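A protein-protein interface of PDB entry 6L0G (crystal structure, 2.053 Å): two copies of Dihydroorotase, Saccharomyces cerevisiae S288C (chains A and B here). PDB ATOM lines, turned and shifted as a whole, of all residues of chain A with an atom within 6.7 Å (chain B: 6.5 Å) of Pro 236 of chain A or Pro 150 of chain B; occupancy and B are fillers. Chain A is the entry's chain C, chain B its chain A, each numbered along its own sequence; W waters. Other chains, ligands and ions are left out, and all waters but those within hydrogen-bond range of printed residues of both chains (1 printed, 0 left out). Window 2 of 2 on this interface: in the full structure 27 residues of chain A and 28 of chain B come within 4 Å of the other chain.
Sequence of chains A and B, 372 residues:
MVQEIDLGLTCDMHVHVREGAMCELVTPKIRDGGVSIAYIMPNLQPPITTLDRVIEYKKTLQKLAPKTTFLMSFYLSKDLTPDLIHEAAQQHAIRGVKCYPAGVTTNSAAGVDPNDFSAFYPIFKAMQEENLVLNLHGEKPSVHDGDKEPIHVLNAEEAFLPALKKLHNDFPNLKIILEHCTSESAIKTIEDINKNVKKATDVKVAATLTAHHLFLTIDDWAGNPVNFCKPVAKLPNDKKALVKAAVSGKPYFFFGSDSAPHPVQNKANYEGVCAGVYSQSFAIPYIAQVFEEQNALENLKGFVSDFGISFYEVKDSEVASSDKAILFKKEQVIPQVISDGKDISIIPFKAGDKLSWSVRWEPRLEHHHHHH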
ATOM      1  N   LEU A 216     -10.664 -11.599   9.780  1.00  0.00           N
ATOM      2  CA  LEU A 216     -10.450 -11.123   8.413  1.00  0.00           C
ATOM      3  C   LEU A 216      -9.257 -11.765   7.718  1.00  0.00           C
ATOM      4  O   LEU A 216      -8.231 -12.078   8.335  1.00  0.00           O
ATOM      5  CB  LEU A 216     -10.225  -9.610   8.401  1.00  0.00           C
ATOM      6  CG  LEU A 216     -11.285  -8.673   8.949  1.00  0.00           C
ATOM      7  CD1 LEU A 216     -10.786  -7.222   8.836  1.00  0.00           C
ATOM      8  CD2 LEU A 216     -12.607  -8.853   8.213  1.00  0.00           C
ATOM      9  N   THR A 217      -9.386 -11.903   6.399  1.00  0.00           N
ATOM     10  CA  THR A 217      -8.290 -12.188   5.486  1.00  0.00           C
ATOM     11  C   THR A 217      -8.369 -11.189   4.332  1.00  0.00           C
ATOM     12  O   THR A 217      -9.276 -10.348   4.258  1.00  0.00           O
ATOM     13  CB  THR A 217      -8.310 -13.630   4.957  1.00  0.00           C
ATOM     14  OG1 THR A 217      -9.488 -13.822   4.178  1.00  0.00           O
ATOM     15  CG2 THR A 217      -8.298 -14.640   6.116  1.00  0.00           C
ATOM     16  N   ILE A 218      -7.375 -11.262   3.448  1.00  0.00           N
ATOM     17  CA  ILE A 218      -7.291 -10.319   2.340  1.00  0.00           C
ATOM     18  C   ILE A 218      -8.604 -10.249   1.563  1.00  0.00           C
ATOM     19  O   ILE A 218      -9.041  -9.166   1.170  1.00  0.00           O
ATOM     20  CB  ILE A 218      -6.100 -10.676   1.429  1.00  0.00           C
ATOM     21  CG1 ILE A 218      -5.956  -9.628   0.328  1.00  0.00           C
ATOM     22  CG2 ILE A 218      -6.254 -12.087   0.860  1.00  0.00           C
ATOM     23  CD1 ILE A 218      -4.542  -9.413  -0.119  1.00  0.00           C
ATOM     24  N   LYS A 234      -4.043 -10.483   6.248  1.00  0.00           N
ATOM     25  CA  LYS A 234      -3.191 -11.191   5.293  1.00  0.00           C
ATOM     26  C   LYS A 234      -3.845 -12.520   4.918  1.00  0.00           C
ATOM     27  O   LYS A 234      -5.034 -12.517   4.574  1.00  0.00           O
ATOM     28  CB  LYS A 234      -1.785 -11.280   5.874  1.00  0.00           C
ATOM     29  CG  LYS A 234      -1.194  -9.877   6.131  1.00  0.00           C
ATOM     30  CD  LYS A 234       0.098  -9.906   6.930  1.00  0.00           C
ATOM     31  CE  LYS A 234       0.807  -8.541   6.873  1.00  0.00           C
ATOM     32  NZ  LYS A 234      -0.088  -7.468   7.418  1.00  0.00           N
ATOM     33  N   LEU A 235      -3.126 -13.642   4.928  1.00  0.00           N
ATOM     34  CA  LEU A 235      -3.600 -14.893   4.348  1.00  0.00           C
ATOM     35  C   LEU A 235      -4.257 -15.790   5.392  1.00  0.00           C
ATOM     36  O   LEU A 235      -4.015 -15.638   6.595  1.00  0.00           O
ATOM     37  CB  LEU A 235      -2.425 -15.628   3.706  1.00  0.00           C
ATOM     38  CG  LEU A 235      -1.737 -14.830   2.598  1.00  0.00           C
ATOM     39  CD1 LEU A 235      -0.650 -15.678   1.935  1.00  0.00           C
ATOM     40  CD2 LEU A 235      -2.766 -14.377   1.580  1.00  0.00           C
ATOM     41  N   PRO A 236      -5.074 -16.762   4.955  1.00  0.00           N
ATOM     42  CA  PRO A 236      -5.641 -17.735   5.909  1.00  0.00           C
ATOM     43  C   PRO A 236      -4.618 -18.348   6.849  1.00  0.00           C
ATOM     44  O   PRO A 236      -4.918 -18.487   8.041  1.00  0.00           O
ATOM     45  CB  PRO A 236      -6.273 -18.788   4.985  1.00  0.00           C
ATOM     46  CG  PRO A 236      -6.674 -18.008   3.776  1.00  0.00           C
ATOM     47  CD  PRO A 236      -5.638 -16.932   3.598  1.00  0.00           C
ATOM     48  N   ASN A 237      -3.401 -18.661   6.376  1.00  0.00           N
ATOM     49  CA  ASN A 237      -2.399 -19.212   7.286  1.00  0.00           C
ATOM     50  C   ASN A 237      -2.035 -18.201   8.366  1.00  0.00           C
ATOM     51  O   ASN A 237      -1.753 -18.583   9.509  1.00  0.00           O
ATOM     52  CB  ASN A 237      -1.147 -19.704   6.536  1.00  0.00           C
ATOM     53  CG  ASN A 237      -0.258 -18.564   5.977  1.00  0.00           C
ATOM     54  OD1 ASN A 237      -0.326 -18.246   4.790  1.00  0.00           O
ATOM     55  ND2 ASN A 237       0.620 -17.994   6.823  1.00  0.00           N
ATOM     56  N   ASP A 238      -2.056 -16.908   8.040  1.00  0.00           N
ATOM     57  CA  ASP A 238      -1.789 -15.909   9.067  1.00  0.00           C
ATOM     58  C   ASP A 238      -2.946 -15.840  10.058  1.00  0.00           C
ATOM     59  O   ASP A 238      -2.730 -15.867  11.271  1.00  0.00           O
ATOM     60  CB  ASP A 238      -1.516 -14.560   8.420  1.00  0.00           C
ATOM     61  CG  ASP A 238      -0.296 -14.610   7.503  1.00  0.00           C
ATOM     62  OD1 ASP A 238       0.830 -14.885   7.973  1.00  0.00           O
ATOM     63  OD2 ASP A 238      -0.477 -14.408   6.301  1.00  0.00           O
ATOM     64  N   LYS A 239      -4.186 -15.766   9.559  1.00  0.00           N
ATOM     65  CA  LYS A 239      -5.338 -15.778  10.450  1.00  0.00           C
ATOM     66  C   LYS A 239      -5.321 -16.978  11.400  1.00  0.00           C
ATOM     67  O   LYS A 239      -5.550 -16.813  12.601  1.00  0.00           O
ATOM     68  CB  LYS A 239      -6.639 -15.773   9.647  1.00  0.00           C
ATOM     69  CG  LYS A 239      -7.856 -15.710  10.547  1.00  0.00           C
ATOM     70  CD  LYS A 239      -9.134 -15.417   9.775  1.00  0.00           C
ATOM     71  CE  LYS A 239      -9.915 -16.685   9.479  1.00  0.00           C
ATOM     72  NZ  LYS A 239     -11.369 -16.413   9.227  1.00  0.00           N
ATOM     73  N   LYS A 240      -5.017 -18.188  10.894  1.00  0.00           N
ATOM     74  CA  LYS A 240      -4.998 -19.349  11.788  1.00  0.00           C
ATOM     75  C   LYS A 240      -3.969 -19.166  12.885  1.00  0.00           C
ATOM     76  O   LYS A 240      -4.259 -19.410  14.055  1.00  0.00           O
ATOM     77  CB  LYS A 240      -4.715 -20.668  11.037  1.00  0.00           C
ATOM     78  CG  LYS A 240      -4.590 -21.901  12.010  1.00  0.00           C
ATOM     79  CD  LYS A 240      -4.194 -23.289  11.384  1.00  0.00           C
ATOM     80  CE  LYS A 240      -3.205 -24.077  12.309  1.00  0.00           C
ATOM     81  NZ  LYS A 240      -3.581 -25.483  12.719  1.00  0.00           N
ATOM     82  N   ALA A 241      -2.772 -18.704  12.535  1.00  0.00           N
ATOM     83  CA  ALA A 241      -1.739 -18.512  13.544  1.00  0.00           C
ATOM     84  C   ALA A 241      -2.119 -17.444  14.575  1.00  0.00           C
ATOM     85  O   ALA A 241      -1.738 -17.559  15.753  1.00  0.00           O
ATOM     86  CB  ALA A 241      -0.411 -18.171  12.868  1.00  0.00           C
ATOM     87  N   SER B 142     -13.289 -17.817  -4.762  1.00  0.00           N
ATOM     88  CA  SER B 142     -12.641 -17.967  -3.466  1.00  0.00           C
ATOM     89  C   SER B 142     -13.297 -19.072  -2.634  1.00  0.00           C
ATOM     90  O   SER B 142     -14.496 -19.345  -2.732  1.00  0.00           O
ATOM     91  CB  SER B 142     -12.666 -16.638  -2.710  1.00  0.00           C
ATOM     92  OG  SER B 142     -11.812 -15.692  -3.341  1.00  0.00           O
ATOM     93  N   VAL B 143     -12.482 -19.715  -1.808  1.00  0.00           N
ATOM     94  CA  VAL B 143     -12.914 -20.815  -0.941  1.00  0.00           C
ATOM     95  C   VAL B 143     -12.164 -20.680   0.371  1.00  0.00           C
ATOM     96  O   VAL B 143     -10.927 -20.662   0.366  1.00  0.00           O
ATOM     97  CB  VAL B 143     -12.621 -22.204  -1.561  1.00  0.00           C
ATOM     98  CG1 VAL B 143     -13.396 -23.300  -0.842  1.00  0.00           C
ATOM     99  CG2 VAL B 143     -12.928 -22.249  -3.066  1.00  0.00           C
ATOM    100  N   HIS B 144     -12.888 -20.583   1.498  1.00  0.00           N
ATOM    101  CA  HIS B 144     -12.126 -20.531   2.746  1.00  0.00           C
ATOM    102  C   HIS B 144     -12.226 -21.930   3.315  1.00  0.00           C
ATOM    103  O   HIS B 144     -11.221 -22.589   3.566  1.00  0.00           O
ATOM    104  CB  HIS B 144     -12.693 -19.587   3.799  1.00  0.00           C
ATOM    105  CG  HIS B 144     -12.689 -18.140   3.422  1.00  0.00           C
ATOM    106  ND1 HIS B 144     -12.955 -17.705   2.140  1.00  0.00           N
ATOM    107  CD2 HIS B 144     -12.153 -17.073   4.067  1.00  0.00           C
ATOM    108  CE1 HIS B 144     -12.844 -16.391   2.095  1.00  0.00           C
ATOM    109  NE2 HIS B 144     -12.304 -15.987   3.234  1.00  0.00           N
ATOM    110  N   ASP B 145     -13.454 -22.316   3.659  1.00  0.00           N
ATOM    111  CA  ASP B 145     -13.821 -23.718   3.811  1.00  0.00           C
ATOM    112  C   ASP B 145     -13.303 -24.412   5.069  1.00  0.00           C
ATOM    113  O   ASP B 145     -14.108 -24.850   5.899  1.00  0.00           O
ATOM    114  CB  ASP B 145     -13.579 -24.451   2.484  1.00  0.00           C
ATOM    115  CG  ASP B 145     -12.173 -25.089   2.324  1.00  0.00           C
ATOM    116  OD1 ASP B 145     -11.184 -24.830   3.027  1.00  0.00           O
ATOM    117  OD2 ASP B 145     -12.116 -25.917   1.394  1.00  0.00           O
ATOM    118  N   GLY B 146     -11.988 -24.509   5.256  1.00  0.00           N
ATOM    119  CA  GLY B 146     -11.439 -25.281   6.352  1.00  0.00           C
ATOM    120  C   GLY B 146     -11.249 -26.772   6.135  1.00  0.00           C
ATOM    121  O   GLY B 146     -11.219 -27.520   7.120  1.00  0.00           O
ATOM    122  N   LYS B 148      -9.891 -27.967   2.339  1.00  0.00           N
ATOM    123  CA  LYS B 148      -8.932 -27.935   1.243  1.00  0.00           C
ATOM    124  C   LYS B 148      -8.358 -26.558   1.080  1.00  0.00           C
ATOM    125  O   LYS B 148      -8.724 -25.588   1.787  1.00  0.00           O
ATOM    126  CB  LYS B 148      -9.415 -28.394  -0.132  1.00  0.00           C
ATOM    127  CG  LYS B 148      -8.201 -29.249  -0.576  1.00  0.00           C
ATOM    128  CD  LYS B 148      -8.261 -30.442  -1.467  1.00  0.00           C
ATOM    129  CE  LYS B 148      -6.767 -30.581  -1.952  1.00  0.00           C
ATOM    130  NZ  LYS B 148      -5.658 -30.585  -0.867  1.00  0.00           N
ATOM    131  N   GLU B 149      -7.419 -26.486   0.149  1.00  0.00           N
ATOM    132  CA  GLU B 149      -6.612 -25.289   0.101  1.00  0.00           C
ATOM    133  C   GLU B 149      -7.434 -24.030  -0.075  1.00  0.00           C
ATOM    134  O   GLU B 149      -8.270 -23.971  -0.954  1.00  0.00           O
ATOM    135  CB  GLU B 149      -5.529 -25.322  -0.944  1.00  0.00           C
ATOM    136  CG  GLU B 149      -4.779 -24.220  -0.392  1.00  0.00           C
ATOM    137  CD  GLU B 149      -3.442 -24.336  -0.204  1.00  0.00           C
ATOM    138  OE1 GLU B 149      -3.173 -25.341   0.519  1.00  0.00           O
ATOM    139  OE2 GLU B 149      -2.681 -23.307  -0.498  1.00  0.00           O
ATOM    140  N   PRO B 150      -7.245 -23.027   0.770  1.00  0.00           N
ATOM    141  CA  PRO B 150      -7.979 -21.781   0.559  1.00  0.00           C
ATOM    142  C   PRO B 150      -7.605 -21.135  -0.783  1.00  0.00           C
ATOM    143  O   PRO B 150      -6.472 -21.222  -1.269  1.00  0.00           O
ATOM    144  CB  PRO B 150      -7.540 -20.912   1.728  1.00  0.00           C
ATOM    145  CG  PRO B 150      -6.963 -21.881   2.714  1.00  0.00           C
ATOM    146  CD  PRO B 150      -6.379 -22.945   1.986  1.00  0.00           C
ATOM    147  N   ILE B 151      -8.606 -20.515  -1.398  1.00  0.00           N
ATOM    148  CA  ILE B 151      -8.452 -19.706  -2.601  1.00  0.00           C
ATOM    149  C   ILE B 151      -8.821 -18.276  -2.233  1.00  0.00           C
ATOM    150  O   ILE B 151      -9.859 -18.053  -1.603  1.00  0.00           O
ATOM    151  CB  ILE B 151      -9.352 -20.198  -3.754  1.00  0.00           C
ATOM    152  CG1 ILE B 151      -9.083 -21.667  -4.096  1.00  0.00           C
ATOM    153  CG2 ILE B 151      -9.156 -19.315  -4.992  1.00  0.00           C
ATOM    154  CD1 ILE B 151      -7.656 -21.963  -4.378  1.00  0.00           C
ATOM    155  N   HIS B 152      -7.965 -17.311  -2.598  1.00  0.00           N
ATOM    156  CA  HIS B 152      -8.209 -15.903  -2.292  1.00  0.00           C
ATOM    157  C   HIS B 152      -7.721 -15.043  -3.463  1.00  0.00           C
ATOM    158  O   HIS B 152      -7.146 -15.539  -4.434  1.00  0.00           O
ATOM    159  CB  HIS B 152      -7.554 -15.516  -0.958  1.00  0.00           C
ATOM    160  CG  HIS B 152      -6.162 -16.038  -0.807  1.00  0.00           C
ATOM    161  ND1 HIS B 152      -5.102 -15.525  -1.518  1.00  0.00           N
ATOM    162  CD2 HIS B 152      -5.658 -17.041  -0.047  1.00  0.00           C
ATOM    163  CE1 HIS B 152      -4.002 -16.185  -1.201  1.00  0.00           C
ATOM    164  NE2 HIS B 152      -4.314 -17.109  -0.308  1.00  0.00           N
ATOM    165  N   ASN B 155      -4.022 -15.810  -4.770  1.00  0.00           N
ATOM    166  CA  ASN B 155      -3.620 -17.036  -5.457  1.00  0.00           C
ATOM    167  C   ASN B 155      -4.678 -17.575  -6.417  1.00  0.00           C
ATOM    168  O   ASN B 155      -4.469 -18.646  -7.001  1.00  0.00           O
ATOM    169  CB  ASN B 155      -3.223 -18.105  -4.433  1.00  0.00           C
ATOM    170  CG  ASN B 155      -4.399 -18.634  -3.636  1.00  0.00           C
ATOM    171  OD1 ASN B 155      -5.540 -18.163  -3.756  1.00  0.00           O
ATOM    172  ND2 ASN B 155      -4.121 -19.615  -2.790  1.00  0.00           N
ATOM    173  N   ALA B 159      -4.219 -20.710  -8.892  1.00  0.00           N
ATOM    174  CA  ALA B 159      -5.135 -21.840  -8.727  1.00  0.00           C
ATOM    175  C   ALA B 159      -5.945 -22.147  -9.987  1.00  0.00           C
ATOM    176  O   ALA B 159      -6.566 -23.210 -10.058  1.00  0.00           O
ATOM    177  CB  ALA B 159      -6.096 -21.574  -7.580  1.00  0.00           C
HETATM  178  O   HOH W   1     -11.682 -14.641   5.691  1.00  0.00           O
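No position is printed for both chains.
Water W1 lies within hydrogen-bond range of OG1 of Thr 217 of chain A (2.8 Å) and NE2 of His 144 of chain B (2.9 Å).
Printed residues of chain B that touch a printed residue of chain A: His 144, Pro 150 and His 152. Along chain B the printed residues that touch a printed residue of chain A span positions 144 to 152. Hydrophobic or aromatic side chains of chain A within 4 Å of the printed part of chain B: Leu 235 and Pro 236. Among the printed residues, 4 pairs touch across the chains. Among the printed residues, no Asp or Glu carboxylate lies within 4 Å of a Lys or Arg side-chain nitrogen of the other chain.
Leu 216 of chain A touches none of the printed residues of chain B. Of the printed residues of chain B, Thr 217 of chain A touches His 144 (3.7 Å). Of the printed residues of chain B, Leu 235 of chain A touches His 152. Pro 236 of chain A touches two residues of chain B. Ile 151 of chain B touches none of the printed residues of chain A. Of the printed residues of chain A, His 152 of chain B touches Leu 235 and Pro 236. The nearest residue of chain B that does not touch Pro 236 of chain A is His 144 of chain B (5.6 Å).
O of Pro 150 of chain B sits at hydrogen-bond distance from ND2 of Asn 155 of chain B (3.2 Å). The backbone NH (N) of His 152 of chain B sits at hydrogen-bond distance from the side-chain amide oxygen (OD1) of Asn 155 of chain B, at 2.8 Å. OD2 of Asp 238 of chain A sits at hydrogen-bond distance from N of Leu 235 of chain A, at 3.1 Å.
Among the printed residues, pairs that only touch across the chains: Leu 235 of chain A with His 152 of chain B, Pro 236 of chain A with His 152 of chain B, Pro 236 of chain A with Pro 150 of chain B and Thr 217 of chain A with His 144 of chain B.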
